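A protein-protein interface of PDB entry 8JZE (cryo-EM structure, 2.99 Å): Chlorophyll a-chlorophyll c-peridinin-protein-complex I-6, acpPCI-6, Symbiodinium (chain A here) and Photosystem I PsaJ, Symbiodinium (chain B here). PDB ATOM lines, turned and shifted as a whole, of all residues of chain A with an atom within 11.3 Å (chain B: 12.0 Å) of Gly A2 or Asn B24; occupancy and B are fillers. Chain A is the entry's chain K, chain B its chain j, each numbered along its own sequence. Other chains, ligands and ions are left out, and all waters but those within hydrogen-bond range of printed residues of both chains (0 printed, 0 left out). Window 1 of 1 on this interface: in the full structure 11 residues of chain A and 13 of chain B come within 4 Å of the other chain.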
ATOM      1  N   GLY A   1       8.991  -0.911 -31.263  1.00  0.00           N
ATOM      2  CA  GLY A   1       8.013  -0.268 -32.121  1.00  0.00           C
ATOM      3  C   GLY A   1       7.412   0.983 -31.511  1.00  0.00           C
ATOM      4  O   GLY A   1       6.747   1.761 -32.195  1.00  0.00           O
ATOM      5  N   GLY A   2       7.647   1.174 -30.215  1.00  0.00           N
ATOM      6  CA  GLY A   2       7.146   2.341 -29.518  1.00  0.00           C
ATOM      7  C   GLY A   2       8.252   3.197 -28.938  1.00  0.00           C
ATOM      8  O   GLY A   2       9.132   3.663 -29.667  1.00  0.00           O
ATOM      9  N   TYR A   3       8.211   3.420 -27.627  1.00  0.00           N
ATOM     10  CA  TYR A   3       9.242   4.211 -26.972  1.00  0.00           C
ATOM     11  C   TYR A   3      10.589   3.502 -27.041  1.00  0.00           C
ATOM     12  O   TYR A   3      10.670   2.272 -27.082  1.00  0.00           O
ATOM     13  CB  TYR A   3       8.869   4.472 -25.511  1.00  0.00           C
ATOM     14  CG  TYR A   3       7.891   5.605 -25.305  1.00  0.00           C
ATOM     15  CD1 TYR A   3       8.340   6.903 -25.100  1.00  0.00           C
ATOM     16  CD2 TYR A   3       6.521   5.378 -25.302  1.00  0.00           C
ATOM     17  CE1 TYR A   3       7.456   7.941 -24.904  1.00  0.00           C
ATOM     18  CE2 TYR A   3       5.628   6.410 -25.107  1.00  0.00           C
ATOM     19  CZ  TYR A   3       6.101   7.690 -24.909  1.00  0.00           C
ATOM     20  OH  TYR A   3       5.215   8.724 -24.716  1.00  0.00           O
ATOM     21  N   LYS A   4      11.658   4.297 -27.061  1.00  0.00           N
ATOM     22  CA  LYS A   4      13.000   3.743 -26.947  1.00  0.00           C
ATOM     23  C   LYS A   4      13.194   3.273 -25.514  1.00  0.00           C
ATOM     24  O   LYS A   4      13.601   4.050 -24.644  1.00  0.00           O
ATOM     25  CB  LYS A   4      14.058   4.780 -27.338  1.00  0.00           C
ATOM     26  CG  LYS A   4      15.494   4.282 -27.259  1.00  0.00           C
ATOM     27  CD  LYS A   4      15.733   3.118 -28.204  1.00  0.00           C
ATOM     28  CE  LYS A   4      17.185   2.669 -28.167  1.00  0.00           C
ATOM     29  NZ  LYS A   4      17.621   2.288 -26.794  1.00  0.00           N
ATOM     30  N   MET A   5      12.889   2.006 -25.258  1.00  0.00           N
ATOM     31  CA  MET A   5      12.858   1.501 -23.894  1.00  0.00           C
ATOM     32  C   MET A   5      14.265   1.417 -23.315  1.00  0.00           C
ATOM     33  O   MET A   5      15.207   0.986 -23.985  1.00  0.00           O
ATOM     34  CB  MET A   5      12.185   0.132 -23.861  1.00  0.00           C
ATOM     35  CG  MET A   5      11.710  -0.293 -22.490  1.00  0.00           C
ATOM     36  SD  MET A   5      10.568   0.882 -21.737  1.00  0.00           S
ATOM     37  CE  MET A   5       9.356   1.079 -23.037  1.00  0.00           C
ATOM     38  N   SER A   6      14.402   1.835 -22.059  1.00  0.00           N
ATOM     39  CA  SER A   6      15.693   1.774 -21.391  1.00  0.00           C
ATOM     40  C   SER A   6      16.116   0.326 -21.197  1.00  0.00           C
ATOM     41  O   SER A   6      15.299  -0.541 -20.877  1.00  0.00           O
ATOM     42  CB  SER A   6      15.636   2.487 -20.040  1.00  0.00           C
ATOM     43  OG  SER A   6      14.925   1.713 -19.090  1.00  0.00           O
ATOM     44  N   PRO A  10      13.683  -2.161 -17.656  1.00  0.00           N
ATOM     45  CA  PRO A  10      12.912  -2.480 -18.869  1.00  0.00           C
ATOM     46  C   PRO A  10      11.493  -1.945 -18.870  1.00  0.00           C
ATOM     47  O   PRO A  10      10.890  -1.854 -19.945  1.00  0.00           O
ATOM     48  CB  PRO A  10      12.924  -4.017 -18.899  1.00  0.00           C
ATOM     49  CG  PRO A  10      14.021  -4.424 -17.967  1.00  0.00           C
ATOM     50  CD  PRO A  10      14.037  -3.374 -16.905  1.00  0.00           C
ATOM     51  N   LEU A  12      10.600   1.104 -17.859  1.00  0.00           N
ATOM     52  CA  LEU A  12      10.618   2.558 -17.918  1.00  0.00           C
ATOM     53  C   LEU A  12      11.310   2.994 -19.204  1.00  0.00           C
ATOM     54  O   LEU A  12      12.425   2.526 -19.498  1.00  0.00           O
ATOM     55  CB  LEU A  12      11.332   3.154 -16.697  1.00  0.00           C
ATOM     56  CG  LEU A  12      10.456   3.913 -15.698  1.00  0.00           C
ATOM     57  CD1 LEU A  12       9.307   3.049 -15.236  1.00  0.00           C
ATOM     58  CD2 LEU A  12      11.272   4.378 -14.510  1.00  0.00           C
ATOM     59  N   PRO A  13      10.691   3.865 -19.999  1.00  0.00           N
ATOM     60  CA  PRO A  13      11.345   4.334 -21.224  1.00  0.00           C
ATOM     61  C   PRO A  13      12.591   5.147 -20.915  1.00  0.00           C
ATOM     62  O   PRO A  13      12.679   5.834 -19.896  1.00  0.00           O
ATOM     63  CB  PRO A  13      10.269   5.198 -21.892  1.00  0.00           C
ATOM     64  CG  PRO A  13       9.398   5.636 -20.771  1.00  0.00           C
ATOM     65  CD  PRO A  13       9.377   4.497 -19.797  1.00  0.00           C
ATOM     66  N   MET A  14      13.566   5.059 -21.818  1.00  0.00           N
ATOM     67  CA  MET A  14      14.828   5.756 -21.620  1.00  0.00           C
ATOM     68  C   MET A  14      14.639   7.260 -21.779  1.00  0.00           C
ATOM     69  O   MET A  14      13.943   7.722 -22.688  1.00  0.00           O
ATOM     70  CB  MET A  14      15.879   5.247 -22.607  1.00  0.00           C
ATOM     71  CG  MET A  14      17.313   5.411 -22.123  1.00  0.00           C
ATOM     72  SD  MET A  14      18.534   4.865 -23.330  1.00  0.00           S
ATOM     73  CE  MET A  14      18.290   6.081 -24.618  1.00  0.00           C
ATOM     74  N   SER A  15      15.259   8.023 -20.884  1.00  0.00           N
ATOM     75  CA  SER A  15      15.145   9.472 -20.941  1.00  0.00           C
ATOM     76  C   SER A  15      15.837  10.004 -22.194  1.00  0.00           C
ATOM     77  O   SER A  15      16.920   9.533 -22.555  1.00  0.00           O
ATOM     78  CB  SER A  15      15.753  10.111 -19.695  1.00  0.00           C
ATOM     79  OG  SER A  15      17.101   9.717 -19.532  1.00  0.00           O
ATOM     80  N   PRO A  16      15.235  10.977 -22.880  1.00  0.00           N
ATOM     81  CA  PRO A  16      15.834  11.479 -24.126  1.00  0.00           C
ATOM     82  C   PRO A  16      17.194  12.126 -23.938  1.00  0.00           C
ATOM     83  O   PRO A  16      17.958  12.213 -24.907  1.00  0.00           O
ATOM     84  CB  PRO A  16      14.798  12.492 -24.631  1.00  0.00           C
ATOM     85  CG  PRO A  16      13.520  12.100 -23.963  1.00  0.00           C
ATOM     86  CD  PRO A  16      13.918  11.581 -22.617  1.00  0.00           C
ATOM     87  N   GLU A  19      20.600  10.083 -24.905  1.00  0.00           N
ATOM     88  CA  GLU A  19      20.895   9.690 -26.276  1.00  0.00           C
ATOM     89  C   GLU A  19      22.252  10.232 -26.710  1.00  0.00           C
ATOM     90  O   GLU A  19      22.565  11.404 -26.484  1.00  0.00           O
ATOM     91  CB  GLU A  19      19.804  10.195 -27.220  1.00  0.00           C
ATOM     92  CG  GLU A  19      18.430   9.596 -26.975  1.00  0.00           C
ATOM     93  CD  GLU A  19      18.304   8.176 -27.495  1.00  0.00           C
ATOM     94  OE1 GLU A  19      19.255   7.685 -28.138  1.00  0.00           O
ATOM     95  OE2 GLU A  19      17.248   7.553 -27.264  1.00  0.00           O
ATOM     96  N   LEU A  36      15.888  14.113 -16.571  1.00  0.00           N
ATOM     97  CA  LEU A  36      14.708  14.841 -17.011  1.00  0.00           C
ATOM     98  C   LEU A  36      14.524  16.162 -16.278  1.00  0.00           C
ATOM     99  O   LEU A  36      13.713  16.985 -16.714  1.00  0.00           O
ATOM    100  CB  LEU A  36      13.458  13.975 -16.823  1.00  0.00           C
ATOM    101  CG  LEU A  36      13.403  12.657 -17.600  1.00  0.00           C
ATOM    102  CD1 LEU A  36      12.220  11.815 -17.160  1.00  0.00           C
ATOM    103  CD2 LEU A  36      13.337  12.918 -19.091  1.00  0.00           C
ATOM    104  N   GLU B   5      11.904  20.096 -30.380  1.00  0.00           N
ATOM    105  CA  GLU B   5      11.042  18.993 -30.806  1.00  0.00           C
ATOM    106  C   GLU B   5       9.990  18.758 -29.724  1.00  0.00           C
ATOM    107  O   GLU B   5      10.227  18.023 -28.761  1.00  0.00           O
ATOM    108  CB  GLU B   5      11.856  17.732 -31.082  1.00  0.00           C
ATOM    109  CG  GLU B   5      12.883  17.381 -30.008  1.00  0.00           C
ATOM    110  CD  GLU B   5      14.204  18.098 -30.192  1.00  0.00           C
ATOM    111  OE1 GLU B   5      14.379  18.763 -31.233  1.00  0.00           O
ATOM    112  OE2 GLU B   5      15.067  17.994 -29.296  1.00  0.00           O
ATOM    113  N   GLY B   6       8.830  19.387 -29.875  1.00  0.00           N
ATOM    114  CA  GLY B   6       7.754  19.172 -28.929  1.00  0.00           C
ATOM    115  C   GLY B   6       6.412  18.928 -29.584  1.00  0.00           C
ATOM    116  O   GLY B   6       5.460  18.511 -28.918  1.00  0.00           O
ATOM    117  N   LEU B   7       6.333  19.167 -30.894  1.00  0.00           N
ATOM    118  CA  LEU B   7       5.068  19.150 -31.625  1.00  0.00           C
ATOM    119  C   LEU B   7       4.040  20.033 -30.922  1.00  0.00           C
ATOM    120  O   LEU B   7       2.892  19.647 -30.698  1.00  0.00           O
ATOM    121  CB  LEU B   7       4.547  17.725 -31.809  1.00  0.00           C
ATOM    122  CG  LEU B   7       4.935  17.055 -33.129  1.00  0.00           C
ATOM    123  CD1 LEU B   7       4.387  17.843 -34.308  1.00  0.00           C
ATOM    124  CD2 LEU B   7       6.443  16.904 -33.248  1.00  0.00           C
ATOM    125  N   ILE B   8       4.484  21.237 -30.563  1.00  0.00           N
ATOM    126  CA  ILE B   8       3.652  22.162 -29.807  1.00  0.00           C
ATOM    127  C   ILE B   8       2.471  22.594 -30.664  1.00  0.00           C
ATOM    128  O   ILE B   8       2.637  22.998 -31.823  1.00  0.00           O
ATOM    129  CB  ILE B   8       4.482  23.368 -29.347  1.00  0.00           C
ATOM    130  CG1 ILE B   8       5.862  22.917 -28.864  1.00  0.00           C
ATOM    131  CG2 ILE B   8       3.773  24.099 -28.237  1.00  0.00           C
ATOM    132  CD1 ILE B   8       5.840  22.171 -27.546  1.00  0.00           C
ATOM    133  N   ILE B  17      -4.518  17.400 -33.805  1.00  0.00           N
ATOM    134  CA  ILE B  17      -3.142  16.993 -34.067  1.00  0.00           C
ATOM    135  C   ILE B  17      -2.820  15.765 -33.225  1.00  0.00           C
ATOM    136  O   ILE B  17      -3.109  15.726 -32.024  1.00  0.00           O
ATOM    137  CB  ILE B  17      -2.167  18.142 -33.768  1.00  0.00           C
ATOM    138  CG1 ILE B  17      -2.567  19.398 -34.545  1.00  0.00           C
ATOM    139  CG2 ILE B  17      -0.744  17.733 -34.115  1.00  0.00           C
ATOM    140  CD1 ILE B  17      -2.544  19.225 -36.046  1.00  0.00           C
ATOM    141  N   THR B  18      -2.224  14.755 -33.858  1.00  0.00           N
ATOM    142  CA  THR B  18      -1.847  13.524 -33.174  1.00  0.00           C
ATOM    143  C   THR B  18      -0.413  13.082 -33.438  1.00  0.00           C
ATOM    144  O   THR B  18       0.119  12.297 -32.644  1.00  0.00           O
ATOM    145  CB  THR B  18      -2.802  12.382 -33.559  1.00  0.00           C
ATOM    146  OG1 THR B  18      -4.143  12.882 -33.603  1.00  0.00           O
ATOM    147  CG2 THR B  18      -2.742  11.252 -32.538  1.00  0.00           C
ATOM    148  N   SER B  19       0.226  13.551 -34.511  1.00  0.00           N
ATOM    149  CA  SER B  19       1.637  13.265 -34.757  1.00  0.00           C
ATOM    150  C   SER B  19       2.454  13.574 -33.513  1.00  0.00           C
ATOM    151  O   SER B  19       2.487  14.717 -33.049  1.00  0.00           O
ATOM    152  CB  SER B  19       2.136  14.090 -35.944  1.00  0.00           C
ATOM    153  OG  SER B  19       2.062  15.478 -35.665  1.00  0.00           O
ATOM    154  N   ARG B  20       3.115  12.551 -32.970  1.00  0.00           N
ATOM    155  CA  ARG B  20       3.582  12.640 -31.587  1.00  0.00           C
ATOM    156  C   ARG B  20       4.835  13.502 -31.449  1.00  0.00           C
ATOM    157  O   ARG B  20       4.780  14.603 -30.893  1.00  0.00           O
ATOM    158  CB  ARG B  20       3.827  11.231 -31.037  1.00  0.00           C
ATOM    159  CG  ARG B  20       2.638  10.289 -31.183  1.00  0.00           C
ATOM    160  CD  ARG B  20       2.926   8.912 -30.594  1.00  0.00           C
ATOM    161  NE  ARG B  20       3.083   8.952 -29.145  1.00  0.00           N
ATOM    162  CZ  ARG B  20       2.094   8.781 -28.278  1.00  0.00           C
ATOM    163  NH1 ARG B  20       0.854   8.555 -28.679  1.00  0.00           N
ATOM    164  NH2 ARG B  20       2.357   8.843 -26.975  1.00  0.00           N
ATOM    165  N   ASP B  21       5.966  13.037 -31.991  1.00  0.00           N
ATOM    166  CA  ASP B  21       7.249  13.697 -31.763  1.00  0.00           C
ATOM    167  C   ASP B  21       8.386  12.964 -32.465  1.00  0.00           C
ATOM    168  O   ASP B  21       8.167  11.919 -33.086  1.00  0.00           O
ATOM    169  CB  ASP B  21       7.551  13.788 -30.263  1.00  0.00           C
ATOM    170  CG  ASP B  21       8.349  15.021 -29.902  1.00  0.00           C
ATOM    171  OD1 ASP B  21       8.791  15.741 -30.822  1.00  0.00           O
ATOM    172  OD2 ASP B  21       8.529  15.274 -28.692  1.00  0.00           O
ATOM    173  N   LYS B  22       9.605  13.509 -32.385  1.00  0.00           N
ATOM    174  CA  LYS B  22      10.780  12.685 -32.650  1.00  0.00           C
ATOM    175  C   LYS B  22      10.935  11.616 -31.575  1.00  0.00           C
ATOM    176  O   LYS B  22      11.406  10.510 -31.861  1.00  0.00           O
ATOM    177  CB  LYS B  22      12.038  13.554 -32.751  1.00  0.00           C
ATOM    178  CG  LYS B  22      12.502  14.185 -31.444  1.00  0.00           C
ATOM    179  CD  LYS B  22      13.669  13.421 -30.830  1.00  0.00           C
ATOM    180  CE  LYS B  22      14.131  14.056 -29.528  1.00  0.00           C
ATOM    181  NZ  LYS B  22      15.218  13.271 -28.877  1.00  0.00           N
ATOM    182  N   ASN B  23      10.554  11.937 -30.341  1.00  0.00           N
ATOM    183  CA  ASN B  23      10.264  10.940 -29.322  1.00  0.00           C
ATOM    184  C   ASN B  23       8.845  10.428 -29.567  1.00  0.00           C
ATOM    185  O   ASN B  23       8.253  10.662 -30.623  1.00  0.00           O
ATOM    186  CB  ASN B  23      10.435  11.534 -27.926  1.00  0.00           C
ATOM    187  CG  ASN B  23      11.832  12.075 -27.686  1.00  0.00           C
ATOM    188  OD1 ASN B  23      12.825  11.463 -28.074  1.00  0.00           O
ATOM    189  ND2 ASN B  23      11.913  13.233 -27.040  1.00  0.00           N
ATOM    190  N   ASN B  24       8.273   9.712 -28.603  1.00  0.00           N
ATOM    191  CA  ASN B  24       6.882   9.291 -28.708  1.00  0.00           C
ATOM    192  C   ASN B  24       5.964  10.105 -27.800  1.00  0.00           C
ATOM    193  O   ASN B  24       4.836   9.684 -27.528  1.00  0.00           O
ATOM    194  CB  ASN B  24       6.751   7.798 -28.413  1.00  0.00           C
ATOM    195  CG  ASN B  24       7.295   6.940 -29.534  1.00  0.00           C
ATOM    196  OD1 ASN B  24       8.182   7.359 -30.276  1.00  0.00           O
ATOM    197  ND2 ASN B  24       6.758   5.735 -29.669  1.00  0.00           N
ATOM    198  N   ASN B  25       6.427  11.255 -27.328  1.00  0.00           N
ATOM    199  CA  ASN B  25       5.598  12.111 -26.491  1.00  0.00           C
ATOM    200  C   ASN B  25       4.449  12.691 -27.309  1.00  0.00           C
ATOM    201  O   ASN B  25       4.670  13.161 -28.430  1.00  0.00           O
ATOM    202  CB  ASN B  25       6.435  13.236 -25.887  1.00  0.00           C
ATOM    203  CG  ASN B  25       7.542  12.721 -24.993  1.00  0.00           C
ATOM    204  OD1 ASN B  25       7.443  11.629 -24.437  1.00  0.00           O
ATOM    205  ND2 ASN B  25       8.602  13.505 -24.847  1.00  0.00           N
ATOM    206  N   PRO B  26       3.224  12.683 -26.791  1.00  0.00           N
ATOM    207  CA  PRO B  26       2.101  13.279 -27.519  1.00  0.00           C
ATOM    208  C   PRO B  26       2.249  14.787 -27.598  1.00  0.00           C
ATOM    209  O   PRO B  26       3.016  15.381 -26.824  1.00  0.00           O
ATOM    210  CB  PRO B  26       0.881  12.876 -26.674  1.00  0.00           C
ATOM    211  CG  PRO B  26       1.428  12.642 -25.312  1.00  0.00           C
ATOM    212  CD  PRO B  26       2.800  12.074 -25.519  1.00  0.00           C
ATOM    213  N   PRO B  27       1.550  15.444 -28.527  1.00  0.00           N
ATOM    214  CA  PRO B  27       1.695  16.899 -28.658  1.00  0.00           C
ATOM    215  C   PRO B  27       1.275  17.627 -27.391  1.00  0.00           C
ATOM    216  O   PRO B  27       0.384  17.189 -26.659  1.00  0.00           O
ATOM    217  CB  PRO B  27       0.774  17.245 -29.835  1.00  0.00           C
ATOM    218  CG  PRO B  27      -0.198  16.117 -29.902  1.00  0.00           C
ATOM    219  CD  PRO B  27       0.583  14.904 -29.496  1.00  0.00           C
ATOM    220  N   ARG B  28       1.939  18.749 -27.134  1.00  0.00           N
ATOM    221  CA  ARG B  28       1.688  19.556 -25.949  1.00  0.00           C
ATOM    222  C   ARG B  28       0.934  20.825 -26.324  1.00  0.00           C
ATOM    223  O   ARG B  28       1.262  21.488 -27.312  1.00  0.00           O
ATOM    224  CB  ARG B  28       2.999  19.921 -25.248  1.00  0.00           C
ATOM    225  CG  ARG B  28       3.831  18.725 -24.814  1.00  0.00           C
ATOM    226  CD  ARG B  28       5.118  19.160 -24.132  1.00  0.00           C
ATOM    227  NE  ARG B  28       4.863  19.990 -22.961  1.00  0.00           N
ATOM    228  CZ  ARG B  28       4.651  19.518 -21.740  1.00  0.00           C
ATOM    229  NH1 ARG B  28       4.656  18.220 -21.489  1.00  0.00           N
ATOM    230  NH2 ARG B  28       4.426  20.372 -20.745  1.00  0.00           N
ATOM    231  N   SER B  44       0.147  18.964 -21.224  1.00  0.00           N
ATOM    232  CA  SER B  44       0.386  17.694 -21.889  1.00  0.00           C
ATOM    233  C   SER B  44      -0.925  17.051 -22.327  1.00  0.00           C
ATOM    234  O   SER B  44      -2.011  17.407 -21.865  1.00  0.00           O
ATOM    235  CB  SER B  44       1.155  16.738 -20.976  1.00  0.00           C
ATOM    236  OG  SER B  44       0.433  16.480 -19.783  1.00  0.00           O
ATOM    237  N   THR B  45      -0.804  16.088 -23.242  1.00  0.00           N
ATOM    238  CA  THR B  45      -1.929  15.309 -23.735  1.00  0.00           C
ATOM    239  C   THR B  45      -1.872  13.855 -23.286  1.00  0.00           C
ATOM    240  O   THR B  45      -2.853  13.124 -23.463  1.00  0.00           O
ATOM    241  CB  THR B  45      -1.980  15.384 -25.271  1.00  0.00           C
ATOM    242  OG1 THR B  45      -1.775  16.740 -25.685  1.00  0.00           O
ATOM    243  CG2 THR B  45      -3.324  14.916 -25.808  1.00  0.00           C
ATOM    244  N   GLY B  46      -0.766  13.425 -22.698  1.00  0.00           N
ATOM    245  CA  GLY B  46      -0.662  12.071 -22.200  1.00  0.00           C
ATOM    246  C   GLY B  46       0.648  11.874 -21.474  1.00  0.00           C
ATOM    247  O   GLY B  46       1.371  12.832 -21.189  1.00  0.00           O
ATOM    248  N   ALA B  47       0.945  10.614 -21.171  1.00  0.00           N
ATOM    249  CA  ALA B  47       2.221  10.288 -20.550  1.00  0.00           C
ATOM    250  C   ALA B  47       3.365  10.626 -21.496  1.00  0.00           C
ATOM    251  O   ALA B  47       3.280  10.398 -22.705  1.00  0.00           O
ATOM    252  CB  ALA B  47       2.266   8.810 -20.170  1.00  0.00           C
ATOM    253  N   SER B  48       4.440  11.180 -20.940  1.00  0.00           N
ATOM    254  CA  SER B  48       5.564  11.618 -21.753  1.00  0.00           C
ATOM    255  C   SER B  48       6.807  11.727 -20.883  1.00  0.00           C
ATOM    256  O   SER B  48       6.720  12.110 -19.714  1.00  0.00           O
ATOM    257  CB  SER B  48       5.265  12.967 -22.417  1.00  0.00           C
ATOM    258  OG  SER B  48       5.014  13.969 -21.447  1.00  0.00           O
ATOM    259  N   ASN B  49       7.958  11.392 -21.459  1.00  0.00           N
ATOM    260  CA  ASN B  49       9.246  11.618 -20.803  1.00  0.00           C
ATOM    261  C   ASN B  49       9.875  12.918 -21.303  1.00  0.00           C
ATOM    262  O   ASN B  49      10.938  12.941 -21.923  1.00  0.00           O
ATOM    263  CB  ASN B  49      10.175  10.422 -21.018  1.00  0.00           C
ATOM    264  CG  ASN B  49      10.352  10.063 -22.483  1.00  0.00           C
ATOM    265  OD1 ASN B  49       9.801  10.716 -23.367  1.00  0.00           O
ATOM    266  ND2 ASN B  49      11.136   9.024 -22.744  1.00  0.00           N
ATOM    267  N   GLN B  50       9.188  14.021 -21.016  1.00  0.00           N
ATOM    268  CA  GLN B  50       9.636  15.332 -21.461  1.00  0.00           C
ATOM    269  C   GLN B  50      10.713  15.875 -20.532  1.00  0.00           C
ATOM    270  O   GLN B  50      10.594  15.802 -19.306  1.00  0.00           O
ATOM    271  CB  GLN B  50       8.458  16.305 -21.527  1.00  0.00           C
ATOM    272  CG  GLN B  50       8.820  17.702 -22.011  1.00  0.00           C
ATOM    273  CD  GLN B  50       9.303  17.722 -23.449  1.00  0.00           C
ATOM    274  OE1 GLN B  50       9.015  16.813 -24.227  1.00  0.00           O
ATOM    275  NE2 GLN B  50      10.044  18.763 -23.808  1.00  0.00           N
ATOM    276  N   VAL B  51      11.771  16.421 -21.126  1.00  0.00           N
ATOM    277  CA  VAL B  51      12.887  16.982 -20.376  1.00  0.00           C
ATOM    278  C   VAL B  51      12.532  18.428 -20.046  1.00  0.00           C
ATOM    279  O   VAL B  51      12.679  19.324 -20.877  1.00  0.00           O
ATOM    280  CB  VAL B  51      14.199  16.885 -21.154  1.00  0.00           C
ATOM    281  CG1 VAL B  51      15.348  17.402 -20.312  1.00  0.00           C
ATOM    282  CG2 VAL B  51      14.451  15.450 -21.580  1.00  0.00           C
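The backbone carbonyl oxygen of Gly A2 lies close to the side-chain amide nitrogen of Asn B24. The backbone carbonyl oxygen (O) of Asn B24 is in hydrogen-bond range of the side-chain hydroxyl (OH) of Tyr A3, 3.0 Å away. OH of Tyr A3 lies within hydrogen-bond range of O of Ala B47 (3.3 Å). The backbone carbonyl oxygen (O) of Met A14 lies within hydrogen-bond range of the side-chain amide nitrogen (ND2) of Asn B49, at 3.1 Å.
Arg B20 touches Tyr A3 (NH2 to OH, 3.6 Å). OH of Tyr A3 touches OD1 of Asn B25 (3.7 Å). Tyr A3 touches Asn B49. ND2 of Asn B23 touches CG of Pro A16 (3.7 Å). Pro A16 touches Asn B49 (CD to O, 3.3 Å). CD2 of Leu A36 touches O of Asn B49, at 3.7 Å. Gln B50 touches Leu A36. Val B51 touches Leu A36 (CG2 to CD2, 3.7 Å).
No residue of chain B comes within 4 Å of Gly A1. Of chain B, only Asn B24 (3.0 Å) comes within 4 Å of Gly A2. Of the printed residues of chain B, Tyr A3 touches Arg B20, Asn B24, Asn B25, Ala B47 and Asn B49. Of the printed residues of chain B, Met A14 touches Asn B49 (3.1 Å). Printed residues of chain B within 4 Å of Pro A16: Asn B23 and Asn B49. Printed residues of chain B within 4 Å of Leu A36: Asn B49 (3.7 Å), Gln B50 (3.99 Å) and Val B51 (3.7 Å). Arg B20 touches just one residue of chain A: Tyr A3. No residue of chain A comes within 4 Å of Asp B21. Asn B25 touches one residue of chain A. No residue of chain A comes within 4 Å of Pro B26. Printed residues of chain A within 4 Å of Gln B50: Leu A36 (3.99 Å). Of the printed residues of chain A, Val B51 touches Leu A36 (3.7 Å). The nearest residue of chain B that does not touch Gly A2 is Asn B23 (6.8 Å).
Of the 14 printed residues of chain A, 5 touch a printed residue of chain B. Hydrophobic or aromatic side chains of chain A that line the printed part of chain B: Tyr A3, Pro A16 and Leu A36. Of the 24 printed residues of chain B, 8 touch a printed residue of chain A. Printed residues of chain B that touch a printed residue of chain A: Arg B20, Asn B23, Asn B24, Asn B25, Ala B47, Asn B49, Gln B50 and Val B51. Among the printed residues, no Asp or Glu carboxylate lies within 4 Å of a Lys or Arg side-chain nitrogen of the other chain.
NE of Arg B20 is in hydrogen-bond range of O of Asn B24 (2.5 Å). NZ of Lys B22 sits at hydrogen-bond distance from OD1 of Asn B23, 3.1 Å away. The side-chain amide oxygen (OD1) of Asn B25 lies close to the side-chain amide oxygen (OD1) of Asn B49 (2.7 Å). ND2 of Asn B25 is in hydrogen-bond range of OE1 of Gln B50 (3.4 Å). The backbone carbonyl oxygen (O) of Lys A4 is in hydrogen-bond range of the backbone NH (N) of Met A14, at 3.0 Å.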
